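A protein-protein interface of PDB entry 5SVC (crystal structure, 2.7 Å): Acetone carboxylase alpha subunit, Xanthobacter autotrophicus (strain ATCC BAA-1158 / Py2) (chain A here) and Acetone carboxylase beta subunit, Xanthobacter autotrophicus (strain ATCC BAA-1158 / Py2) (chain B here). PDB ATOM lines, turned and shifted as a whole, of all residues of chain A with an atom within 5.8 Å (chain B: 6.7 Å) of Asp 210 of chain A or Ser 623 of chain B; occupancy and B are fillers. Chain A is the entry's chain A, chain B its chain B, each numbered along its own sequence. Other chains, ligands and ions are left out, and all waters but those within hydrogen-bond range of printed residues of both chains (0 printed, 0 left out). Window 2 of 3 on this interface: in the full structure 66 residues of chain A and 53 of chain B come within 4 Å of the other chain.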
ATOM      1  N   ASP A 135      29.863  20.041  -9.024  1.00  0.00           N
ATOM      2  CA  ASP A 135      28.536  19.788  -8.476  1.00  0.00           C
ATOM      3  C   ASP A 135      28.592  18.592  -7.525  1.00  0.00           C
ATOM      4  O   ASP A 135      29.443  17.701  -7.645  1.00  0.00           O
ATOM      5  CB  ASP A 135      27.527  19.550  -9.606  1.00  0.00           C
ATOM      6  CG  ASP A 135      26.077  19.704  -9.148  1.00  0.00           C
ATOM      7  OD1 ASP A 135      25.830  20.446  -8.150  1.00  0.00           O
ATOM      8  OD2 ASP A 135      25.189  19.101  -9.818  1.00  0.00           O
ATOM      9  N   LYS A 136      27.720  18.603  -6.526  1.00  0.00           N
ATOM     10  CA  LYS A 136      27.600  17.490  -5.601  1.00  0.00           C
ATOM     11  C   LYS A 136      28.829  17.358  -4.701  1.00  0.00           C
ATOM     12  O   LYS A 136      28.847  16.475  -3.847  1.00  0.00           O
ATOM     13  CB  LYS A 136      27.338  16.161  -6.338  1.00  0.00           C
ATOM     14  CG  LYS A 136      25.858  15.876  -6.795  1.00  0.00           C
ATOM     15  CD  LYS A 136      25.079  17.132  -7.219  1.00  0.00           C
ATOM     16  CE  LYS A 136      23.569  16.993  -6.977  1.00  0.00           C
ATOM     17  NZ  LYS A 136      22.870  18.294  -7.258  1.00  0.00           N
ATOM     18  N   ASP A 137      29.858  18.195  -4.869  1.00  0.00           N
ATOM     19  CA  ASP A 137      31.005  18.200  -3.968  1.00  0.00           C
ATOM     20  C   ASP A 137      30.591  18.672  -2.564  1.00  0.00           C
ATOM     21  O   ASP A 137      29.514  19.241  -2.379  1.00  0.00           O
ATOM     22  CB  ASP A 137      32.112  19.090  -4.526  1.00  0.00           C
ATOM     23  CG  ASP A 137      33.062  18.351  -5.468  1.00  0.00           C
ATOM     24  OD1 ASP A 137      32.975  17.108  -5.623  1.00  0.00           O
ATOM     25  OD2 ASP A 137      33.941  19.031  -6.034  1.00  0.00           O
ATOM     26  N   ILE A 138      31.464  18.441  -1.565  1.00  0.00           N
ATOM     27  CA  ILE A 138      31.230  18.831  -0.163  1.00  0.00           C
ATOM     28  C   ILE A 138      32.510  19.375   0.461  1.00  0.00           C
ATOM     29  O   ILE A 138      33.486  18.632   0.621  1.00  0.00           O
ATOM     30  CB  ILE A 138      30.751  17.664   0.723  1.00  0.00           C
ATOM     31  CG1 ILE A 138      29.524  16.960   0.164  1.00  0.00           C
ATOM     32  CG2 ILE A 138      30.521  18.166   2.162  1.00  0.00           C
ATOM     33  CD1 ILE A 138      29.173  15.727   0.947  1.00  0.00           C
ATOM     34  N   GLY A 207      33.783  15.554   0.476  1.00  0.00           N
ATOM     35  CA  GLY A 207      32.936  14.626  -0.230  1.00  0.00           C
ATOM     36  C   GLY A 207      32.932  14.974  -1.693  1.00  0.00           C
ATOM     37  O   GLY A 207      33.344  16.066  -2.099  1.00  0.00           O
ATOM     38  N   ALA A 208      32.513  13.991  -2.487  1.00  0.00           N
ATOM     39  CA  ALA A 208      32.131  14.164  -3.885  1.00  0.00           C
ATOM     40  C   ALA A 208      30.898  13.314  -4.151  1.00  0.00           C
ATOM     41  O   ALA A 208      30.593  12.368  -3.415  1.00  0.00           O
ATOM     42  CB  ALA A 208      33.245  13.759  -4.862  1.00  0.00           C
ATOM     43  N   ASN A 209      30.216  13.637  -5.238  1.00  0.00           N
ATOM     44  CA  ASN A 209      28.953  12.999  -5.583  1.00  0.00           C
ATOM     45  C   ASN A 209      28.127  12.747  -4.328  1.00  0.00           C
ATOM     46  O   ASN A 209      27.661  11.641  -4.059  1.00  0.00           O
ATOM     47  CB  ASN A 209      29.165  11.715  -6.374  1.00  0.00           C
ATOM     48  CG  ASN A 209      27.878  11.249  -7.038  1.00  0.00           C
ATOM     49  OD1 ASN A 209      27.008  12.071  -7.360  1.00  0.00           O
ATOM     50  ND2 ASN A 209      27.746   9.937  -7.256  1.00  0.00           N
ATOM     51  N   ASP A 210      28.017  13.794  -3.516  1.00  0.00           N
ATOM     52  CA  ASP A 210      27.128  13.879  -2.367  1.00  0.00           C
ATOM     53  C   ASP A 210      27.489  12.919  -1.229  1.00  0.00           C
ATOM     54  O   ASP A 210      26.716  12.780  -0.264  1.00  0.00           O
ATOM     55  CB  ASP A 210      25.689  13.663  -2.841  1.00  0.00           C
ATOM     56  CG  ASP A 210      24.993  14.966  -3.228  1.00  0.00           C
ATOM     57  OD1 ASP A 210      25.657  16.027  -3.451  1.00  0.00           O
ATOM     58  OD2 ASP A 210      23.749  14.920  -3.304  1.00  0.00           O
ATOM     59  N   THR A 211      28.680  12.327  -1.261  1.00  0.00           N
ATOM     60  CA  THR A 211      29.064  11.278  -0.331  1.00  0.00           C
ATOM     61  C   THR A 211      30.398  11.590   0.331  1.00  0.00           C
ATOM     62  O   THR A 211      31.344  11.986  -0.357  1.00  0.00           O
ATOM     63  CB  THR A 211      29.157   9.975  -1.072  1.00  0.00           C
ATOM     64  OG1 THR A 211      28.047   9.878  -1.967  1.00  0.00           O
ATOM     65  CG2 THR A 211      29.122   8.832  -0.118  1.00  0.00           C
ATOM     66  N   LEU A 212      30.487  11.369   1.655  1.00  0.00           N
ATOM     67  CA  LEU A 212      31.688  11.708   2.412  1.00  0.00           C
ATOM     68  C   LEU A 212      32.836  10.726   2.186  1.00  0.00           C
ATOM     69  O   LEU A 212      32.637   9.548   1.889  1.00  0.00           O
ATOM     70  CB  LEU A 212      31.374  11.779   3.894  1.00  0.00           C
ATOM     71  CG  LEU A 212      30.399  12.889   4.299  1.00  0.00           C
ATOM     72  CD1 LEU A 212      30.108  12.778   5.765  1.00  0.00           C
ATOM     73  CD2 LEU A 212      30.954  14.272   4.007  1.00  0.00           C
ATOM     74  N   ARG A 235      26.010  15.551  10.081  1.00  0.00           N
ATOM     75  CA  ARG A 235      24.743  15.315   9.396  1.00  0.00           C
ATOM     76  C   ARG A 235      23.780  16.492   9.560  1.00  0.00           C
ATOM     77  O   ARG A 235      22.958  16.752   8.675  1.00  0.00           O
ATOM     78  CB  ARG A 235      24.070  14.024   9.901  1.00  0.00           C
ATOM     79  CG  ARG A 235      24.922  12.776   9.812  1.00  0.00           C
ATOM     80  CD  ARG A 235      25.297  12.367   8.398  1.00  0.00           C
ATOM     81  NE  ARG A 235      26.365  11.359   8.417  1.00  0.00           N
ATOM     82  CZ  ARG A 235      26.979  10.855   7.340  1.00  0.00           C
ATOM     83  NH1 ARG A 235      26.647  11.246   6.109  1.00  0.00           N
ATOM     84  NH2 ARG A 235      27.933   9.945   7.494  1.00  0.00           N
ATOM     85  N   ILE A 238      25.147  18.909   6.670  1.00  0.00           N
ATOM     86  CA  ILE A 238      24.902  18.354   5.349  1.00  0.00           C
ATOM     87  C   ILE A 238      23.415  18.361   5.015  1.00  0.00           C
ATOM     88  O   ILE A 238      23.015  18.754   3.910  1.00  0.00           O
ATOM     89  CB  ILE A 238      25.520  16.952   5.273  1.00  0.00           C
ATOM     90  CG1 ILE A 238      27.021  17.128   5.524  1.00  0.00           C
ATOM     91  CG2 ILE A 238      25.277  16.361   3.926  1.00  0.00           C
ATOM     92  CD1 ILE A 238      27.838  15.897   5.317  1.00  0.00           C
ATOM     93  N   ALA A 239      22.569  17.933   5.959  1.00  0.00           N
ATOM     94  CA  ALA A 239      21.132  17.916   5.682  1.00  0.00           C
ATOM     95  C   ALA A 239      20.592  19.319   5.429  1.00  0.00           C
ATOM     96  O   ALA A 239      19.697  19.508   4.592  1.00  0.00           O
ATOM     97  CB  ALA A 239      20.360  17.275   6.830  1.00  0.00           C
ATOM     98  N   HIS A 242      21.818  20.625   1.929  1.00  0.00           N
ATOM     99  CA  HIS A 242      21.087  19.987   0.842  1.00  0.00           C
ATOM    100  C   HIS A 242      19.614  20.328   0.848  1.00  0.00           C
ATOM    101  O   HIS A 242      19.004  20.372  -0.222  1.00  0.00           O
ATOM    102  CB  HIS A 242      21.271  18.478   0.886  1.00  0.00           C
ATOM    103  CG  HIS A 242      22.636  18.051   0.479  1.00  0.00           C
ATOM    104  ND1 HIS A 242      23.054  16.741   0.520  1.00  0.00           N
ATOM    105  CD2 HIS A 242      23.684  18.773   0.016  1.00  0.00           C
ATOM    106  CE1 HIS A 242      24.308  16.674   0.102  1.00  0.00           C
ATOM    107  NE2 HIS A 242      24.711  17.893  -0.214  1.00  0.00           N
ATOM    108  N   ARG A 245      20.023  23.637  -1.055  1.00  0.00           N
ATOM    109  CA  ARG A 245      20.358  23.465  -2.464  1.00  0.00           C
ATOM    110  C   ARG A 245      19.124  23.063  -3.262  1.00  0.00           C
ATOM    111  O   ARG A 245      18.829  23.637  -4.320  1.00  0.00           O
ATOM    112  CB  ARG A 245      21.478  22.427  -2.605  1.00  0.00           C
ATOM    113  CG  ARG A 245      21.818  22.006  -4.044  1.00  0.00           C
ATOM    114  CD  ARG A 245      22.955  20.958  -4.112  1.00  0.00           C
ATOM    115  NE  ARG A 245      22.575  19.650  -3.590  1.00  0.00           N
ATOM    116  CZ  ARG A 245      23.393  18.597  -3.510  1.00  0.00           C
ATOM    117  NH1 ARG A 245      24.655  18.678  -3.933  1.00  0.00           N
ATOM    118  NH2 ARG A 245      22.944  17.453  -3.003  1.00  0.00           N
ATOM    119  N   GLY B 617      15.647   9.931   4.802  1.00  0.00           N
ATOM    120  CA  GLY B 617      16.096  10.652   3.630  1.00  0.00           C
ATOM    121  C   GLY B 617      15.108  11.718   3.202  1.00  0.00           C
ATOM    122  O   GLY B 617      15.493  12.845   2.874  1.00  0.00           O
ATOM    123  N   TYR B 620      14.724  14.576   5.885  1.00  0.00           N
ATOM    124  CA  TYR B 620      15.879  15.447   5.937  1.00  0.00           C
ATOM    125  C   TYR B 620      16.519  15.504   4.565  1.00  0.00           C
ATOM    126  O   TYR B 620      16.182  16.368   3.749  1.00  0.00           O
ATOM    127  CB  TYR B 620      16.880  14.975   7.000  1.00  0.00           C
ATOM    128  CG  TYR B 620      16.305  14.931   8.399  1.00  0.00           C
ATOM    129  CD1 TYR B 620      16.126  16.101   9.135  1.00  0.00           C
ATOM    130  CD2 TYR B 620      15.938  13.722   8.991  1.00  0.00           C
ATOM    131  CE1 TYR B 620      15.593  16.077  10.432  1.00  0.00           C
ATOM    132  CE2 TYR B 620      15.387  13.692  10.285  1.00  0.00           C
ATOM    133  CZ  TYR B 620      15.222  14.874  10.995  1.00  0.00           C
ATOM    134  OH  TYR B 620      14.699  14.859  12.264  1.00  0.00           O
ATOM    135  N   ALA B 621      17.455  14.597   4.328  1.00  0.00           N
ATOM    136  CA  ALA B 621      18.228  14.541   3.098  1.00  0.00           C
ATOM    137  C   ALA B 621      18.989  13.234   3.070  1.00  0.00           C
ATOM    138  O   ALA B 621      19.533  12.816   4.075  1.00  0.00           O
ATOM    139  CB  ALA B 621      19.194  15.720   3.005  1.00  0.00           C
ATOM    140  N   ALA B 622      19.003  12.597   1.928  1.00  0.00           N
ATOM    141  CA  ALA B 622      19.709  11.343   1.722  1.00  0.00           C
ATOM    142  C   ALA B 622      21.073  11.332   2.392  1.00  0.00           C
ATOM    143  O   ALA B 622      21.479  10.312   2.948  1.00  0.00           O
ATOM    144  CB  ALA B 622      19.855  11.073   0.215  1.00  0.00           C
ATOM    145  N   SER B 623      21.794  12.452   2.330  1.00  0.00           N
ATOM    146  CA  SER B 623      23.144  12.522   2.896  1.00  0.00           C
ATOM    147  C   SER B 623      23.152  12.808   4.408  1.00  0.00           C
ATOM    148  O   SER B 623      24.210  12.734   5.046  1.00  0.00           O
ATOM    149  CB  SER B 623      23.945  13.573   2.130  1.00  0.00           C
ATOM    150  OG  SER B 623      23.770  13.368   0.724  1.00  0.00           O
ATOM    151  N   ALA B 624      21.989  13.071   5.004  1.00  0.00           N
ATOM    152  CA  ALA B 624      21.852  13.097   6.456  1.00  0.00           C
ATOM    153  C   ALA B 624      22.007  11.710   7.077  1.00  0.00           C
ATOM    154  O   ALA B 624      22.228  11.617   8.286  1.00  0.00           O
ATOM    155  CB  ALA B 624      20.488  13.687   6.850  1.00  0.00           C
ATOM    156  N   ARG B 625      21.874  10.643   6.289  1.00  0.00           N
ATOM    157  CA  ARG B 625      21.796   9.283   6.818  1.00  0.00           C
ATOM    158  C   ARG B 625      23.134   8.829   7.395  1.00  0.00           C
ATOM    159  O   ARG B 625      24.173   8.924   6.726  1.00  0.00           O
ATOM    160  CB  ARG B 625      21.363   8.312   5.719  1.00  0.00           C
ATOM    161  CG  ARG B 625      19.910   8.377   5.309  1.00  0.00           C
ATOM    162  CD  ARG B 625      19.570   7.113   4.541  1.00  0.00           C
ATOM    163  NE  ARG B 625      18.520   7.337   3.554  1.00  0.00           N
ATOM    164  CZ  ARG B 625      18.748   7.561   2.258  1.00  0.00           C
ATOM    165  NH1 ARG B 625      19.999   7.592   1.796  1.00  0.00           N
ATOM    166  NH2 ARG B 625      17.728   7.758   1.424  1.00  0.00           N
ATOM    167  N   SER B 626      23.093   8.299   8.627  1.00  0.00           N
ATOM    168  CA  SER B 626      24.281   7.873   9.373  1.00  0.00           C
ATOM    169  C   SER B 626      24.117   6.442   9.876  1.00  0.00           C
ATOM    170  O   SER B 626      24.216   6.175  11.075  1.00  0.00           O
ATOM    171  CB  SER B 626      24.547   8.815  10.543  1.00  0.00           C
ATOM    172  OG  SER B 626      23.387   8.939  11.337  1.00  0.00           O
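The backbone carbonyl oxygen of Asp 210 of chain A is in hydrogen-bond range of the side-chain hydroxyl of Ser 623 of chain B (3.2 Å).
The guanidinium group (NH1) of Arg 235 of chain A sits at hydrogen-bond distance from the backbone carbonyl oxygen (O) of Ser 623 of chain B, 3.0 Å away.
The side-chain hydroxyl of Ser 623 of chain B lies close to a ring nitrogen (ND1) of His 242 of chain A, at 3.5 Å.
The guanidinium group (NH1) of Arg 235 of chain A is in hydrogen-bond range of the backbone carbonyl oxygen (O) of Arg 625 of chain B (3.4 Å).
NH1 of Arg 625 of chain B is in hydrogen-bond range of O of Ala 622 of chain B (3.3 Å).
N of Asp 210 of chain A is in hydrogen-bond range of O of Lys 136 of chain A, 2.8 Å away.
NH2 of Arg 245 of chain A lies within salt-bridge range of OD2 of Asp 210 of chain A (2.7 Å).
A ring nitrogen (NE2) of His 242 of chain A lies within hydrogen-bond range of the guanidinium group of Arg 245 of chain A (3.3 Å).
Among the printed residues, merely in contact across the chains: Arg 235 of chain A with Ala 624 of chain B, Arg 235 of chain A with Ser 626 of chain B, Ile 238 of chain A with Ser 623 of chain B, Ala 239 of chain A with Ala 621 of chain B and Ala 239 of chain A with Ala 624 of chain B.
Ser 623 of chain B touches just these residues of chain A: Asp 210, Arg 235, Ile 238 and His 242.
Printed residues of chain B within 4 Å of His 242 of chain A: Ser 623.
Printed residues of chain A within 4 Å of Arg 625 of chain B: Arg 235.
Of the printed residues of chain B, Ile 238 of chain A touches Ser 623 (3.6 Å).
Printed residues of chain B within 4 Å of Ala 239 of chain A: Ala 621 (3.97 Å) and Ala 624 (3.6 Å).
The nearest printed residue of chain A that does not touch Ser 623 of chain B is Ala 239 of chain A (5.4 Å).
Of the 8 printed residues of chain B, 5 touch a printed residue of chain A.
Hydrophobic or aromatic side chains of chain B that line the printed part of chain A: Ala 621 and Ala 624.
Along chain B the printed residues that touch a printed residue of chain A span positions 621 to 626.
Hydrophobic or aromatic side chains of chain A within 4 Å of the printed part of chain B: Ile 238, Ala 239 and His 242.
Among the printed residues, 9 pairs touch across the chains.
Among the printed residues, no Asp or Glu carboxylate lies within 4 Å of a Lys or Arg side-chain nitrogen of the other chain.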
